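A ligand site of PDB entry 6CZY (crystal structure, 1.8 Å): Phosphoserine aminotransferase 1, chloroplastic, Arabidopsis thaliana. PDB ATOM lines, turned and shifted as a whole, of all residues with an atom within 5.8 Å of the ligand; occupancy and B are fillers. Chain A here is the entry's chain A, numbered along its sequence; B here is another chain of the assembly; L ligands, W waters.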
ATOM      1  N   ALA A  10     -20.266 -13.855  33.601  1.00  0.00           N
ATOM      2  CA  ALA A  10     -19.901 -15.101  32.920  1.00  0.00           C
ATOM      3  C   ALA A  10     -18.407 -15.434  33.017  1.00  0.00           C
ATOM      4  O   ALA A  10     -17.985 -16.461  32.516  1.00  0.00           O
ATOM      5  CB  ALA A  10     -20.316 -15.053  31.436  1.00  0.00           C
ATOM      6  N   GLY A  11     -17.615 -14.532  33.590  1.00  0.00           N
ATOM      7  CA  GLY A  11     -16.188 -14.765  33.780  1.00  0.00           C
ATOM      8  C   GLY A  11     -15.443 -13.485  33.503  1.00  0.00           C
ATOM      9  O   GLY A  11     -15.611 -12.931  32.434  1.00  0.00           O
ATOM     10  N   GLY A  75      -1.802 -16.537  30.915  1.00  0.00           N
ATOM     11  CA  GLY A  75      -2.089 -16.405  29.492  1.00  0.00           C
ATOM     12  C   GLY A  75      -3.514 -16.681  29.089  1.00  0.00           C
ATOM     13  O   GLY A  75      -3.900 -16.428  27.937  1.00  0.00           O
ATOM     14  N   GLY A  76      -4.282 -17.232  30.010  1.00  0.00           N
ATOM     15  CA  GLY A  76      -5.668 -17.664  29.759  1.00  0.00           C
ATOM     16  C   GLY A  76      -5.817 -18.896  28.913  1.00  0.00           C
ATOM     17  O   GLY A  76      -4.852 -19.388  28.371  1.00  0.00           O
ATOM     18  N   ALA A  77      -7.052 -19.377  28.766  1.00  0.00           N
ATOM     19  CA  ALA A  77      -7.316 -20.451  27.828  1.00  0.00           C
ATOM     20  C   ALA A  77      -6.866 -20.082  26.403  1.00  0.00           C
ATOM     21  O   ALA A  77      -6.512 -20.978  25.606  1.00  0.00           O
ATOM     22  CB  ALA A  77      -8.761 -20.837  27.853  1.00  0.00           C
ATOM     23  N   THR A  78      -6.976 -18.816  26.031  1.00  0.00           N
ATOM     24  CA  THR A  78      -6.606 -18.414  24.646  1.00  0.00           C
ATOM     25  C   THR A  78      -5.157 -18.724  24.304  1.00  0.00           C
ATOM     26  O   THR A  78      -4.845 -19.055  23.158  1.00  0.00           O
ATOM     27  CB  THR A  78      -6.961 -16.933  24.388  1.00  0.00           C
ATOM     28  OG1 THR A  78      -8.346 -16.768  24.632  1.00  0.00           O
ATOM     29  CG2 THR A  78      -6.756 -16.622  22.920  1.00  0.00           C
ATOM     30  N   THR A  79      -4.273 -18.681  25.295  1.00  0.00           N
ATOM     31  CA  THR A  79      -2.840 -18.975  25.048  1.00  0.00           C
ATOM     32  C   THR A  79      -2.757 -20.468  24.770  1.00  0.00           C
ATOM     33  O   THR A  79      -1.995 -20.898  23.935  1.00  0.00           O
ATOM     34  CB  THR A  79      -1.954 -18.542  26.219  1.00  0.00           C
ATOM     35  OG1 THR A  79      -1.918 -17.090  26.304  1.00  0.00           O
ATOM     36  CG2 THR A  79      -0.580 -19.112  26.138  1.00  0.00           C
ATOM     37  N   PHE A  81      -4.925 -22.266  23.192  1.00  0.00           N
ATOM     38  CA  PHE A  81      -5.343 -22.523  21.830  1.00  0.00           C
ATOM     39  C   PHE A  81      -4.088 -22.621  20.918  1.00  0.00           C
ATOM     40  O   PHE A  81      -4.108 -23.343  19.912  1.00  0.00           O
ATOM     41  CB  PHE A  81      -6.292 -21.441  21.302  1.00  0.00           C
ATOM     42  CG  PHE A  81      -7.617 -21.318  22.022  1.00  0.00           C
ATOM     43  CD1 PHE A  81      -8.138 -22.343  22.766  1.00  0.00           C
ATOM     44  CD2 PHE A  81      -8.409 -20.173  21.804  1.00  0.00           C
ATOM     45  CE1 PHE A  81      -9.380 -22.214  23.368  1.00  0.00           C
ATOM     46  CE2 PHE A  81      -9.664 -20.047  22.400  1.00  0.00           C
ATOM     47  CZ  PHE A  81     -10.142 -21.070  23.169  1.00  0.00           C
ATOM     48  N   TRP A 103     -16.476 -20.717  21.334  1.00  0.00           N
ATOM     49  CA  TRP A 103     -15.163 -20.980  21.925  1.00  0.00           C
ATOM     50  C   TRP A 103     -14.382 -22.066  21.181  1.00  0.00           C
ATOM     51  O   TRP A 103     -13.160 -21.896  20.920  1.00  0.00           O
ATOM     52  CB  TRP A 103     -15.229 -21.234  23.431  1.00  0.00           C
ATOM     53  CG  TRP A 103     -15.582 -19.951  24.135  1.00  0.00           C
ATOM     54  CD1 TRP A 103     -16.740 -19.650  24.813  1.00  0.00           C
ATOM     55  CD2 TRP A 103     -14.789 -18.766  24.159  1.00  0.00           C
ATOM     56  NE1 TRP A 103     -16.692 -18.356  25.274  1.00  0.00           N
ATOM     57  CE2 TRP A 103     -15.495 -17.802  24.892  1.00  0.00           C
ATOM     58  CE3 TRP A 103     -13.547 -18.441  23.615  1.00  0.00           C
ATOM     59  CZ2 TRP A 103     -14.981 -16.502  25.101  1.00  0.00           C
ATOM     60  CZ3 TRP A 103     -13.030 -17.172  23.844  1.00  0.00           C
ATOM     61  CH2 TRP A 103     -13.744 -16.232  24.542  1.00  0.00           C
ATOM     62  N   CYS A 149     -15.025 -28.355  23.323  1.00  0.00           N
ATOM     63  CA  CYS A 149     -15.225 -27.379  24.413  1.00  0.00           C
ATOM     64  C   CYS A 149     -16.362 -27.951  25.218  1.00  0.00           C
ATOM     65  O   CYS A 149     -17.495 -28.075  24.724  1.00  0.00           O
ATOM     66  CB  CYS A 149     -15.561 -26.016  23.834  1.00  0.00           C
ATOM     67  SG  CYS A 149     -15.933 -24.811  25.152  1.00  0.00           S
ATOM     68  N   ASN A 151     -18.028 -27.076  27.873  1.00  0.00           N
ATOM     69  CA  ASN A 151     -19.101 -26.175  28.214  1.00  0.00           C
ATOM     70  C   ASN A 151     -18.923 -24.895  27.419  1.00  0.00           C
ATOM     71  O   ASN A 151     -17.991 -24.118  27.663  1.00  0.00           O
ATOM     72  CB  ASN A 151     -19.159 -25.917  29.712  1.00  0.00           C
ATOM     73  CG  ASN A 151     -20.394 -25.142  30.122  1.00  0.00           C
ATOM     74  OD1 ASN A 151     -21.502 -25.717  30.253  1.00  0.00           O
ATOM     75  ND2 ASN A 151     -20.233 -23.818  30.300  1.00  0.00           N
ATOM     76  N   GLU A 152     -19.832 -24.679  26.443  1.00  0.00           N
ATOM     77  CA  GLU A 152     -19.759 -23.518  25.561  1.00  0.00           C
ATOM     78  C   GLU A 152     -20.492 -22.365  26.238  1.00  0.00           C
ATOM     79  O   GLU A 152     -21.725 -22.336  26.282  1.00  0.00           O
ATOM     80  CB  GLU A 152     -20.336 -23.862  24.191  1.00  0.00           C
ATOM     81  CG  GLU A 152     -19.293 -24.509  23.312  1.00  0.00           C
ATOM     82  CD  GLU A 152     -18.284 -23.533  22.689  1.00  0.00           C
ATOM     83  OE1 GLU A 152     -18.356 -22.330  22.975  1.00  0.00           O
ATOM     84  OE2 GLU A 152     -17.429 -23.997  21.894  1.00  0.00           O
ATOM     85  N   THR A 153     -19.693 -21.469  26.815  1.00  0.00           N
ATOM     86  CA  THR A 153     -20.136 -20.475  27.788  1.00  0.00           C
ATOM     87  C   THR A 153     -21.195 -19.493  27.273  1.00  0.00           C
ATOM     88  O   THR A 153     -22.037 -19.018  28.026  1.00  0.00           O
ATOM     89  CB  THR A 153     -18.881 -19.686  28.217  1.00  0.00           C
ATOM     90  OG1 THR A 153     -17.816 -20.598  28.375  1.00  0.00           O
ATOM     91  CG2 THR A 153     -19.078 -18.986  29.570  1.00  0.00           C
ATOM     92  N   ASP A 173     -11.504 -28.216  26.542  1.00  0.00           N
ATOM     93  CA  ASP A 173     -11.579 -26.894  27.206  1.00  0.00           C
ATOM     94  C   ASP A 173     -12.721 -26.960  28.187  1.00  0.00           C
ATOM     95  O   ASP A 173     -13.882 -26.870  27.762  1.00  0.00           O
ATOM     96  CB  ASP A 173     -11.868 -25.802  26.128  1.00  0.00           C
ATOM     97  CG  ASP A 173     -12.038 -24.425  26.662  1.00  0.00           C
ATOM     98  OD1 ASP A 173     -11.982 -24.227  27.897  1.00  0.00           O
ATOM     99  OD2 ASP A 173     -12.288 -23.526  25.792  1.00  0.00           O
ATOM    100  N   MET A 174     -12.372 -27.056  29.474  1.00  0.00           N
ATOM    101  CA  MET A 174     -13.371 -27.030  30.547  1.00  0.00           C
ATOM    102  C   MET A 174     -13.353 -25.744  31.324  1.00  0.00           C
ATOM    103  O   MET A 174     -13.761 -25.748  32.506  1.00  0.00           O
ATOM    104  CB  MET A 174     -13.153 -28.215  31.482  1.00  0.00           C
ATOM    105  CG  MET A 174     -13.412 -29.549  30.781  1.00  0.00           C
ATOM    106  SD  MET A 174     -13.225 -30.970  31.890  1.00  0.00           S
ATOM    107  CE  MET A 174     -14.063 -32.222  30.910  1.00  0.00           C
ATOM    108  N   SER A 175     -12.943 -24.641  30.687  1.00  0.00           N
ATOM    109  CA  SER A 175     -12.897 -23.349  31.397  1.00  0.00           C
ATOM    110  C   SER A 175     -14.165 -23.060  32.201  1.00  0.00           C
ATOM    111  O   SER A 175     -14.075 -22.637  33.361  1.00  0.00           O
ATOM    112  CB  SER A 175     -12.706 -22.164  30.428  1.00  0.00           C
ATOM    113  OG  SER A 175     -11.465 -22.230  29.703  1.00  0.00           O
ATOM    114  N   SER A 176     -15.340 -23.154  31.579  1.00  0.00           N
ATOM    115  CA  SER A 176     -16.540 -22.682  32.279  1.00  0.00           C
ATOM    116  C   SER A 176     -17.332 -23.797  32.981  1.00  0.00           C
ATOM    117  O   SER A 176     -18.386 -23.511  33.512  1.00  0.00           O
ATOM    118  CB  SER A 176     -17.441 -21.855  31.344  1.00  0.00           C
ATOM    119  OG  SER A 176     -17.726 -22.617  30.148  1.00  0.00           O
ATOM    120  N   GLY A 194      -9.234 -21.667  32.012  1.00  0.00           N
ATOM    121  CA  GLY A 194      -9.001 -20.483  32.873  1.00  0.00           C
ATOM    122  C   GLY A 194      -9.705 -20.674  34.210  1.00  0.00           C
ATOM    123  O   GLY A 194     -10.741 -21.350  34.298  1.00  0.00           O
ATOM    124  N   GLN A 196     -11.021 -18.356  36.083  1.00  0.00           N
ATOM    125  CA  GLN A 196     -11.945 -17.299  36.363  1.00  0.00           C
ATOM    126  C   GLN A 196     -13.472 -17.578  36.315  1.00  0.00           C
ATOM    127  O   GLN A 196     -14.245 -16.642  36.392  1.00  0.00           O
ATOM    128  CB  GLN A 196     -11.581 -16.064  35.537  1.00  0.00           C
ATOM    129  CG  GLN A 196     -11.833 -16.175  34.044  1.00  0.00           C
ATOM    130  CD  GLN A 196     -10.627 -16.659  33.267  1.00  0.00           C
ATOM    131  OE1 GLN A 196      -9.711 -17.306  33.815  1.00  0.00           O
ATOM    132  NE2 GLN A 196     -10.628 -16.365  31.963  1.00  0.00           N
ATOM    133  N   LYS A 197     -13.935 -18.818  36.125  1.00  0.00           N
ATOM    134  CA  LYS A 197     -15.361 -19.103  36.308  1.00  0.00           C
ATOM    135  C   LYS A 197     -15.663 -19.783  37.567  1.00  0.00           C
ATOM    136  O   LYS A 197     -16.483 -19.297  38.379  1.00  0.00           O
ATOM    137  CB  LYS A 197     -15.852 -19.976  35.139  1.00  0.00           C
ATOM    138  CG  LYS A 197     -15.819 -19.280  33.794  1.00  0.00           C
ATOM    139  CD  LYS A 197     -14.385 -19.163  33.269  1.00  0.00           C
ATOM    140  CE  LYS A 197     -14.297 -18.813  31.817  1.00  0.00           C
ATOM    141  NZ  LYS A 197     -15.405 -17.921  31.421  1.00  0.00           N
ATOM    142  N   THR A 205      -4.419 -20.150  34.579  1.00  0.00           N
ATOM    143  CA  THR A 205      -4.967 -21.162  33.679  1.00  0.00           C
ATOM    144  C   THR A 205      -4.416 -22.511  34.138  1.00  0.00           C
ATOM    145  O   THR A 205      -3.217 -22.584  34.476  1.00  0.00           O
ATOM    146  CB  THR A 205      -4.491 -20.882  32.242  1.00  0.00           C
ATOM    147  OG1 THR A 205      -4.999 -19.597  31.835  1.00  0.00           O
ATOM    148  CG2 THR A 205      -4.961 -21.944  31.269  1.00  0.00           C
ATOM    149  N   GLN B  74      -0.464 -10.572  30.382  1.00  0.00           N
ATOM    150  CA  GLN B  74      -0.001 -11.683  31.165  1.00  0.00           C
ATOM    151  C   GLN B  74       1.198 -12.321  30.501  1.00  0.00           C
ATOM    152  O   GLN B  74       1.514 -12.053  29.349  1.00  0.00           O
ATOM    153  CB  GLN B  74      -1.069 -12.789  31.242  1.00  0.00           C
ATOM    154  CG  GLN B  74      -2.464 -12.337  31.551  1.00  0.00           C
ATOM    155  CD  GLN B  74      -3.419 -13.517  31.677  1.00  0.00           C
ATOM    156  OE1 GLN B  74      -3.118 -14.518  32.338  1.00  0.00           O
ATOM    157  NE2 GLN B  74      -4.598 -13.390  31.006  1.00  0.00           N
ATOM    158  N   MET B 224      -2.275 -14.345  21.346  1.00  0.00           N
ATOM    159  CA  MET B 224      -2.062 -13.783  22.672  1.00  0.00           C
ATOM    160  C   MET B 224      -0.711 -13.094  22.799  1.00  0.00           C
ATOM    161  O   MET B 224      -0.484 -12.437  23.803  1.00  0.00           O
ATOM    162  CB  MET B 224      -2.232 -14.824  23.767  1.00  0.00           C
ATOM    163  CG  MET B 224      -3.653 -15.224  24.073  1.00  0.00           C
ATOM    164  SD  MET B 224      -4.666 -13.815  24.547  1.00  0.00           S
ATOM    165  CE  MET B 224      -3.769 -13.237  25.992  1.00  0.00           C
ATOM    166  N   ASN B 238      -8.728 -10.947  25.455  1.00  0.00           N
ATOM    167  CA  ASN B 238      -9.245 -12.016  26.282  1.00  0.00           C
ATOM    168  C   ASN B 238      -9.423 -11.499  27.687  1.00  0.00           C
ATOM    169  O   ASN B 238      -9.463 -10.298  27.873  1.00  0.00           O
ATOM    170  CB  ASN B 238      -8.358 -13.274  26.261  1.00  0.00           C
ATOM    171  CG  ASN B 238      -7.061 -13.113  27.051  1.00  0.00           C
ATOM    172  OD1 ASN B 238      -6.510 -12.007  27.180  1.00  0.00           O
ATOM    173  ND2 ASN B 238      -6.567 -14.246  27.596  1.00  0.00           N
ATOM    174  N   THR B 239      -9.581 -12.415  28.667  1.00  0.00           N
ATOM    175  CA  THR B 239      -9.739 -12.001  30.034  1.00  0.00           C
ATOM    176  C   THR B 239      -8.412 -11.538  30.624  1.00  0.00           C
ATOM    177  O   THR B 239      -7.486 -12.311  30.739  1.00  0.00           O
ATOM    178  CB  THR B 239     -10.368 -13.110  30.884  1.00  0.00           C
ATOM    179  OG1 THR B 239     -11.418 -13.770  30.161  1.00  0.00           O
ATOM    180  CG2 THR B 239     -10.968 -12.446  32.128  1.00  0.00           C
HETATM  181  N1  LIG L   1     -12.980 -21.076  26.577  1.00  0.00           N
HETATM  182  C1  LIG L   1     -14.130 -20.837  27.238  1.00  0.00           C
HETATM  183  C2  LIG L   1     -15.160 -21.972  27.391  1.00  0.00           C
HETATM  184  C3  LIG L   1     -14.323 -19.560  27.791  1.00  0.00           C
HETATM  185  O1  LIG L   1     -15.506 -19.317  28.478  1.00  0.00           O
HETATM  186  C4  LIG L   1     -13.378 -18.573  27.628  1.00  0.00           C
HETATM  187  C5  LIG L   1     -13.564 -17.180  28.257  1.00  0.00           C
HETATM  188  N2  LIG L   1     -14.957 -16.876  28.503  1.00  0.00           N
HETATM  189  C6  LIG L   1     -12.221 -18.850  26.956  1.00  0.00           C
HETATM  190  C7  LIG L   1     -12.038 -20.138  26.423  1.00  0.00           C
HETATM  191  C8  LIG L   1     -11.106 -17.827  26.771  1.00  0.00           C
HETATM  192  O2  LIG L   1     -10.428 -17.747  28.021  1.00  0.00           O
HETATM  193  P1  LIG L   1      -9.418 -16.539  28.412  1.00  0.00           P
HETATM  194  O3  LIG L   1      -8.319 -16.572  27.342  1.00  0.00           O
HETATM  195  O4  LIG L   1      -8.809 -16.883  29.744  1.00  0.00           O
HETATM  196  O5  LIG L   1     -10.163 -15.240  28.357  1.00  0.00           O
HETATM  197  O   HOH W   1     -16.906 -15.913  29.759  1.00  0.00           O
HETATM  198  O   HOH W   2     -11.763 -14.258  26.349  1.00  0.00           O
HETATM  199  O   HOH W   3     -13.715 -15.060  31.070  1.00  0.00           O
HETATM  200  O   HOH W   4      -7.145 -15.026  30.903  1.00  0.00           O
HETATM  201  O   HOH W   5     -10.931 -19.467  30.355  1.00  0.00           O
HETATM  202  O   HOH W   6     -18.151 -16.226  27.456  1.00  0.00           O
HETATM  203  O   HOH W   7     -15.805 -24.882  29.127  1.00  0.00           O
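ND2 of Asn 238 of chain B is in hydrogen-bond range of O of Gly 75.
The side-chain amide nitrogen (NE2) of Gln 196 sits at hydrogen-bond distance from the side-chain hydroxyl (OG1) of Thr 239 of chain B (3.3 Å).
O of Asn 151 sits at hydrogen-bond distance from SG of Cys 149.
OG of Ser 175 is in hydrogen-bond range of N of Gly 194 (3.3 Å).
The backbone carbonyl oxygen of Thr 239 of chain B lies within hydrogen-bond range of the side-chain amide nitrogen of Gln 74 of chain B.
The side-chain amino group of Lys 197 sits at hydrogen-bond distance from the backbone carbonyl oxygen of Ala 10, 3.2 Å away.
SG of Cys 149 lies close to OE2 of Glu 152, 3.7 Å away.
The side-chain hydroxyl (OG) of Ser 175 lies within hydrogen-bond range of the side-chain carboxylate (OD1) of Asp 173.
The backbone NH (N) of Ala 77 sits at hydrogen-bond distance from an oxygen (O4) of the ligand (3.2 Å).
The side-chain hydroxyl (OG1) of Thr 153 sits at hydrogen-bond distance from an oxygen (O1) of the ligand, at 2.6 Å.
OD2 of Asp 173 sits at hydrogen-bond distance from N1 of the ligand.
The side-chain amino group (NZ) of Lys 197 is in hydrogen-bond range of an oxygen (O1) of the ligand, at 3.3 Å.
An oxygen (O3) of the ligand lies within hydrogen-bond range of the side-chain amide nitrogen (ND2) of Asn 238 of chain B.
The side-chain hydroxyl (OG1) of Thr 78 sits at hydrogen-bond distance from an oxygen (O3) of the ligand.
O3 of the ligand sits at hydrogen-bond distance from N of Thr 78, 2.9 Å away.
The backbone NH of Thr 239 of chain B sits at hydrogen-bond distance from an oxygen (O5) of the ligand, at 2.9 Å.
The side-chain amide nitrogen (NE2) of Gln 196 is in hydrogen-bond range of an oxygen (O4) of the ligand (2.9 Å).
An oxygen (O5) of the ligand is in hydrogen-bond range of the side-chain hydroxyl (OG1) of Thr 239 of chain B (2.6 Å).
Gly 76 touches the ligand (CA to O4, 3.2 Å).
Phe 81 touches the ligand (CZ to C7, 3.9 Å).
CZ2 of Trp 103 touches N2 of the ligand, 3.4 Å away.
Cys 149 touches the ligand (SG to C2, 3.7 Å).
Asn 151 touches the ligand.
Ser 175 touches the ligand (OG to N1, 3.7 Å).
OG of Ser 176 touches C2 of the ligand, 3.8 Å away.
Hydrophobic or aromatic side chains within 4 Å of the ligand: Ala 77, Phe 81 and Trp 103.
15 residues have an atom within 4 Å of the ligand: Gly 76, Ala 77, Thr 78, Phe 81, Trp 103, Cys 149, Asn 151, Thr 153, Asp 173, Ser 175, Ser 176, Gln 196, Lys 197, Asn 238 of chain B and Thr 239 of chain B.
Water W1 lies within hydrogen-bond range of a nitrogen (N2) of the ligand (2.5 Å), the side-chain amino group of Lys 197 (3.0 Å) and the backbone carbonyl oxygen of Ala 10 (3.0 Å).
Water W4 lies within hydrogen-bond range of O of Thr 239 of chain B, O4 of the ligand, NE2 of Gln 74 of chain B and ND2 of Asn 238 of chain B.
Water W5 lies within hydrogen-bond range of OG of Ser 175 (2.9 Å), O2 of the ligand (2.9 Å) and N of Gly 194 (3.2 Å).
Water W3 lies within hydrogen-bond range of OG1 of Thr 239 of chain B (2.8 Å), O of Gly 11 (3.2 Å), NZ of Lys 197 (3.3 Å), N2 of the ligand (3.4 Å) and NE2 of Gln 196 (3.5 Å).
Water W6 lies within hydrogen-bond range of the indole nitrogen of Trp 103 (3.4 Å) and a nitrogen (N2) of the ligand (3.4 Å).
Water W7 lies within hydrogen-bond range of the backbone carbonyl oxygen of Asn 151 (2.7 Å), the backbone NH of Ser 176 (3.0 Å), the backbone carbonyl oxygen of Asp 173 (3.1 Å) and the backbone NH of Ser 175 (3.3 Å).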
